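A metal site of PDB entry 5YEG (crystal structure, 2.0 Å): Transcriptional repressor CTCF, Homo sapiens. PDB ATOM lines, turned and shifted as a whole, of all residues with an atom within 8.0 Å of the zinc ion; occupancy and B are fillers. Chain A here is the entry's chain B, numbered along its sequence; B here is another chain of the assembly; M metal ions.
A ring nitrogen (ND1) of His 77 lies within hydrogen-bond range of OP1 of DA 10 of chain B, 2.7 Å away.
SG of Cys 64 lies close to N of Ala 66 (3.6 Å).
SG of Cys 61 sits close to N of Ile 63 (3.4 Å).
The backbone NH (N) of Cys 61 sits at hydrogen-bond distance from the backbone carbonyl oxygen (O) of Ala 66, at 2.8 Å.
SD of Met 74 is in hydrogen-bond range of N of Cys 61, 3.8 Å away.
The zinc ion is bound by a ring nitrogen (NE2) of His 77 (2.1 Å).
NE2 of His 82 is bound to the zinc ion, at 2.2 Å.
SG of Cys 64 is bound to the zinc ion, 2.3 Å away.
SG of Cys 61 is bound to the zinc ion, at 2.3 Å.
Within 4 Å of the zinc ion: Cys 61, Cys 64, His 77 and His 82.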
ATOM      1  N   GLU A  60       1.381 -27.924 -22.347  1.00  0.00           N
ATOM      2  CA  GLU A  60       2.631 -27.415 -22.877  1.00  0.00           C
ATOM      3  C   GLU A  60       2.505 -27.165 -24.370  1.00  0.00           C
ATOM      4  O   GLU A  60       2.113 -28.065 -25.123  1.00  0.00           O
ATOM      5  CB  GLU A  60       3.772 -28.416 -22.608  1.00  0.00           C
ATOM      6  CG  GLU A  60       5.082 -28.032 -23.288  1.00  0.00           C
ATOM      7  CD  GLU A  60       6.236 -28.967 -22.928  1.00  0.00           C
ATOM      8  OE1 GLU A  60       6.008 -29.940 -22.171  1.00  0.00           O
ATOM      9  OE2 GLU A  60       7.370 -28.718 -23.389  1.00  0.00           O
ATOM     10  N   CYS A  61       2.843 -25.951 -24.794  1.00  0.00           N
ATOM     11  CA  CYS A  61       2.816 -25.659 -26.227  1.00  0.00           C
ATOM     12  C   CYS A  61       3.844 -26.542 -26.924  1.00  0.00           C
ATOM     13  O   CYS A  61       5.031 -26.514 -26.589  1.00  0.00           O
ATOM     14  CB  CYS A  61       3.109 -24.180 -26.480  1.00  0.00           C
ATOM     15  SG  CYS A  61       3.404 -23.815 -28.239  1.00  0.00           S
ATOM     16  N   TYR A  62       3.380 -27.355 -27.869  1.00  0.00           N
ATOM     17  CA  TYR A  62       4.295 -28.296 -28.507  1.00  0.00           C
ATOM     18  C   TYR A  62       5.366 -27.602 -29.347  1.00  0.00           C
ATOM     19  O   TYR A  62       6.361 -28.229 -29.713  1.00  0.00           O
ATOM     20  CB  TYR A  62       3.498 -29.300 -29.357  1.00  0.00           C
ATOM     21  CG  TYR A  62       3.046 -28.771 -30.714  1.00  0.00           C
ATOM     22  CD1 TYR A  62       1.871 -28.045 -30.853  1.00  0.00           C
ATOM     23  CD2 TYR A  62       3.790 -29.039 -31.860  1.00  0.00           C
ATOM     24  CE1 TYR A  62       1.464 -27.581 -32.097  1.00  0.00           C
ATOM     25  CE2 TYR A  62       3.384 -28.575 -33.104  1.00  0.00           C
ATOM     26  CZ  TYR A  62       2.227 -27.858 -33.225  1.00  0.00           C
ATOM     27  OH  TYR A  62       1.829 -27.397 -34.469  1.00  0.00           O
ATOM     28  N   ILE A  63       5.170 -26.320 -29.682  1.00  0.00           N
ATOM     29  CA  ILE A  63       6.155 -25.601 -30.501  1.00  0.00           C
ATOM     30  C   ILE A  63       7.231 -24.935 -29.655  1.00  0.00           C
ATOM     31  O   ILE A  63       8.425 -25.163 -29.864  1.00  0.00           O
ATOM     32  CB  ILE A  63       5.412 -24.588 -31.406  1.00  0.00           C
ATOM     33  CG1 ILE A  63       4.569 -25.331 -32.460  1.00  0.00           C
ATOM     34  CG2 ILE A  63       6.400 -23.619 -32.064  1.00  0.00           C
ATOM     35  CD1 ILE A  63       3.562 -24.434 -33.156  1.00  0.00           C
ATOM     36  N   CYS A  64       6.855 -24.114 -28.669  1.00  0.00           N
ATOM     37  CA  CYS A  64       7.823 -23.318 -27.937  1.00  0.00           C
ATOM     38  C   CYS A  64       7.978 -23.732 -26.479  1.00  0.00           C
ATOM     39  O   CYS A  64       8.835 -23.172 -25.777  1.00  0.00           O
ATOM     40  CB  CYS A  64       7.450 -21.828 -28.002  1.00  0.00           C
ATOM     41  SG  CYS A  64       6.131 -21.349 -26.898  1.00  0.00           S
ATOM     42  N   HIS A  65       7.150 -24.681 -26.016  1.00  0.00           N
ATOM     43  CA  HIS A  65       7.232 -25.333 -24.717  1.00  0.00           C
ATOM     44  C   HIS A  65       6.843 -24.441 -23.548  1.00  0.00           C
ATOM     45  O   HIS A  65       7.062 -24.828 -22.388  1.00  0.00           O
ATOM     46  CB  HIS A  65       8.631 -25.932 -24.503  1.00  0.00           C
ATOM     47  CG  HIS A  65       9.086 -26.787 -25.644  1.00  0.00           C
ATOM     48  ND1 HIS A  65       8.525 -28.017 -25.916  1.00  0.00           N
ATOM     49  CD2 HIS A  65      10.014 -26.581 -26.603  1.00  0.00           C
ATOM     50  CE1 HIS A  65       9.102 -28.542 -26.974  1.00  0.00           C
ATOM     51  NE2 HIS A  65      10.012 -27.698 -27.421  1.00  0.00           N
ATOM     52  N   ALA A  66       6.227 -23.285 -23.811  1.00  0.00           N
ATOM     53  CA  ALA A  66       5.540 -22.551 -22.764  1.00  0.00           C
ATOM     54  C   ALA A  66       4.436 -23.419 -22.164  1.00  0.00           C
ATOM     55  O   ALA A  66       3.909 -24.324 -22.800  1.00  0.00           O
ATOM     56  CB  ALA A  66       4.947 -21.269 -23.331  1.00  0.00           C
ATOM     57  N   ARG A  67       4.122 -23.165 -20.898  1.00  0.00           N
ATOM     58  CA  ARG A  67       3.230 -24.015 -20.118  1.00  0.00           C
ATOM     59  C   ARG A  67       2.018 -23.226 -19.642  1.00  0.00           C
ATOM     60  O   ARG A  67       2.079 -22.007 -19.454  1.00  0.00           O
ATOM     61  CB  ARG A  67       4.021 -24.646 -18.971  1.00  0.00           C
ATOM     62  CG  ARG A  67       5.079 -25.644 -19.483  1.00  0.00           C
ATOM     63  CD  ARG A  67       5.669 -26.499 -18.375  1.00  0.00           C
ATOM     64  NE  ARG A  67       4.716 -27.477 -17.869  1.00  0.00           N
ATOM     65  CZ  ARG A  67       4.533 -28.688 -18.382  1.00  0.00           C
ATOM     66  NH1 ARG A  67       5.246 -29.092 -19.419  1.00  0.00           N
ATOM     67  NH2 ARG A  67       3.636 -29.501 -17.829  1.00  0.00           N
ATOM     68  N   PHE A  68       0.884 -23.928 -19.482  1.00  0.00           N
ATOM     69  CA  PHE A  68      -0.387 -23.270 -19.199  1.00  0.00           C
ATOM     70  C   PHE A  68      -1.172 -24.071 -18.156  1.00  0.00           C
ATOM     71  O   PHE A  68      -0.977 -25.276 -18.032  1.00  0.00           O
ATOM     72  CB  PHE A  68      -1.172 -23.117 -20.509  1.00  0.00           C
ATOM     73  CG  PHE A  68      -0.387 -22.410 -21.567  1.00  0.00           C
ATOM     74  CD1 PHE A  68       0.438 -23.123 -22.435  1.00  0.00           C
ATOM     75  CD2 PHE A  68      -0.402 -21.016 -21.648  1.00  0.00           C
ATOM     76  CE1 PHE A  68       1.215 -22.452 -23.387  1.00  0.00           C
ATOM     77  CE2 PHE A  68       0.364 -20.339 -22.609  1.00  0.00           C
ATOM     78  CZ  PHE A  68       1.168 -21.058 -23.469  1.00  0.00           C
ATOM     79  N   MET A  74      -3.771 -22.777 -23.777  1.00  0.00           N
ATOM     80  CA  MET A  74      -2.679 -23.160 -24.670  1.00  0.00           C
ATOM     81  C   MET A  74      -3.113 -23.048 -26.120  1.00  0.00           C
ATOM     82  O   MET A  74      -2.333 -22.596 -26.974  1.00  0.00           O
ATOM     83  CB  MET A  74      -2.211 -24.572 -24.358  1.00  0.00           C
ATOM     84  CG  MET A  74      -1.244 -25.165 -25.407  1.00  0.00           C
ATOM     85  SD  MET A  74      -0.809 -26.847 -24.946  1.00  0.00           S
ATOM     86  CE  MET A  74      -2.358 -27.682 -25.282  1.00  0.00           C
ATOM     87  N   HIS A  77      -2.956 -19.504 -27.063  1.00  0.00           N
ATOM     88  CA  HIS A  77      -1.560 -19.123 -27.235  1.00  0.00           C
ATOM     89  C   HIS A  77      -1.035 -19.559 -28.604  1.00  0.00           C
ATOM     90  O   HIS A  77      -0.347 -18.794 -29.291  1.00  0.00           O
ATOM     91  CB  HIS A  77      -0.714 -19.744 -26.126  1.00  0.00           C
ATOM     92  CG  HIS A  77       0.745 -19.800 -26.434  1.00  0.00           C
ATOM     93  ND1 HIS A  77       1.627 -18.825 -26.042  1.00  0.00           N
ATOM     94  CD2 HIS A  77       1.460 -20.704 -27.142  1.00  0.00           C
ATOM     95  CE1 HIS A  77       2.838 -19.141 -26.466  1.00  0.00           C
ATOM     96  NE2 HIS A  77       2.770 -20.280 -27.137  1.00  0.00           N
ATOM     97  N   ILE A  78      -1.356 -20.783 -29.011  1.00  0.00           N
ATOM     98  CA  ILE A  78      -0.884 -21.256 -30.307  1.00  0.00           C
ATOM     99  C   ILE A  78      -1.508 -20.440 -31.431  1.00  0.00           C
ATOM    100  O   ILE A  78      -0.833 -20.042 -32.397  1.00  0.00           O
ATOM    101  CB  ILE A  78      -1.155 -22.764 -30.452  1.00  0.00           C
ATOM    102  CG1 ILE A  78      -0.239 -23.544 -29.497  1.00  0.00           C
ATOM    103  CG2 ILE A  78      -0.897 -23.202 -31.919  1.00  0.00           C
ATOM    104  CD1 ILE A  78      -0.580 -25.005 -29.324  1.00  0.00           C
ATOM    105  N   LEU A  79      -2.795 -20.137 -31.294  1.00  0.00           N
ATOM    106  CA  LEU A  79      -3.492 -19.326 -32.300  1.00  0.00           C
ATOM    107  C   LEU A  79      -2.853 -17.958 -32.450  1.00  0.00           C
ATOM    108  O   LEU A  79      -2.716 -17.451 -33.574  1.00  0.00           O
ATOM    109  CB  LEU A  79      -4.962 -19.184 -31.908  1.00  0.00           C
ATOM    110  CG  LEU A  79      -5.870 -18.503 -32.928  1.00  0.00           C
ATOM    111  CD1 LEU A  79      -5.943 -19.317 -34.218  1.00  0.00           C
ATOM    112  CD2 LEU A  79      -7.251 -18.329 -32.327  1.00  0.00           C
ATOM    113  N   LYS A  81       0.305 -16.847 -31.346  1.00  0.00           N
ATOM    114  CA  LYS A  81       1.748 -16.738 -31.518  1.00  0.00           C
ATOM    115  C   LYS A  81       2.324 -17.579 -32.665  1.00  0.00           C
ATOM    116  O   LYS A  81       3.402 -17.242 -33.165  1.00  0.00           O
ATOM    117  CB  LYS A  81       2.483 -17.138 -30.226  1.00  0.00           C
ATOM    118  CG  LYS A  81       1.958 -16.439 -28.968  1.00  0.00           C
ATOM    119  CD  LYS A  81       2.023 -14.925 -29.100  1.00  0.00           C
ATOM    120  CE  LYS A  81       3.445 -14.457 -29.400  1.00  0.00           C
ATOM    121  NZ  LYS A  81       3.548 -12.966 -29.403  1.00  0.00           N
ATOM    122  N   HIS A  82       1.683 -18.687 -33.062  1.00  0.00           N
ATOM    123  CA  HIS A  82       2.286 -19.623 -34.010  1.00  0.00           C
ATOM    124  C   HIS A  82       1.416 -19.892 -35.235  1.00  0.00           C
ATOM    125  O   HIS A  82       1.613 -20.894 -35.920  1.00  0.00           O
ATOM    126  CB  HIS A  82       2.622 -20.955 -33.325  1.00  0.00           C
ATOM    127  CG  HIS A  82       3.470 -20.817 -32.100  1.00  0.00           C
ATOM    128  ND1 HIS A  82       4.698 -20.191 -32.117  1.00  0.00           N
ATOM    129  CD2 HIS A  82       3.256 -21.186 -30.816  1.00  0.00           C
ATOM    130  CE1 HIS A  82       5.217 -20.218 -30.905  1.00  0.00           C
ATOM    131  NE2 HIS A  82       4.353 -20.795 -30.093  1.00  0.00           N
ATOM    132  P    DA B  10       0.149 -16.329 -23.550  1.00  0.00           P
ATOM    133  OP1  DA B  10       1.338 -17.094 -23.993  1.00  0.00           O
ATOM    134  OP2  DA B  10      -1.118 -16.498 -24.304  1.00  0.00           O
ATOM    135  O5'  DA B  10      -0.153 -16.662 -22.040  1.00  0.00           O
ATOM    136  C5'  DA B  10       0.872 -16.510 -21.072  1.00  0.00           C
ATOM    137  C4'  DA B  10       0.286 -16.579 -19.690  1.00  0.00           C
ATOM    138  O4'  DA B  10      -0.743 -15.560 -19.568  1.00  0.00           O
ATOM    139  C3'  DA B  10      -0.395 -17.903 -19.321  1.00  0.00           C
ATOM    140  O3'  DA B  10      -0.130 -18.199 -17.964  1.00  0.00           O
ATOM    141  C2'  DA B  10      -1.869 -17.623 -19.586  1.00  0.00           C
ATOM    142  C1'  DA B  10      -1.979 -16.138 -19.231  1.00  0.00           C
ATOM    143  N9   DA B  10      -3.036 -15.482 -19.985  1.00  0.00           N
ATOM    144  C8   DA B  10      -3.344 -15.669 -21.296  1.00  0.00           C
ATOM    145  N7   DA B  10      -4.390 -14.975 -21.710  1.00  0.00           N
ATOM    146  C5   DA B  10      -4.805 -14.314 -20.577  1.00  0.00           C
ATOM    147  C6   DA B  10      -5.878 -13.436 -20.347  1.00  0.00           C
ATOM    148  N6   DA B  10      -6.734 -13.048 -21.309  1.00  0.00           N
ATOM    149  N1   DA B  10      -6.026 -12.936 -19.100  1.00  0.00           N
ATOM    150  C2   DA B  10      -5.160 -13.326 -18.148  1.00  0.00           C
ATOM    151  N3   DA B  10      -4.122 -14.160 -18.240  1.00  0.00           N
ATOM    152  C4   DA B  10      -4.005 -14.628 -19.493  1.00  0.00           C
HETATM  153 ZN    ZN M   1       4.162 -21.635 -28.050  1.00  0.00          ZN
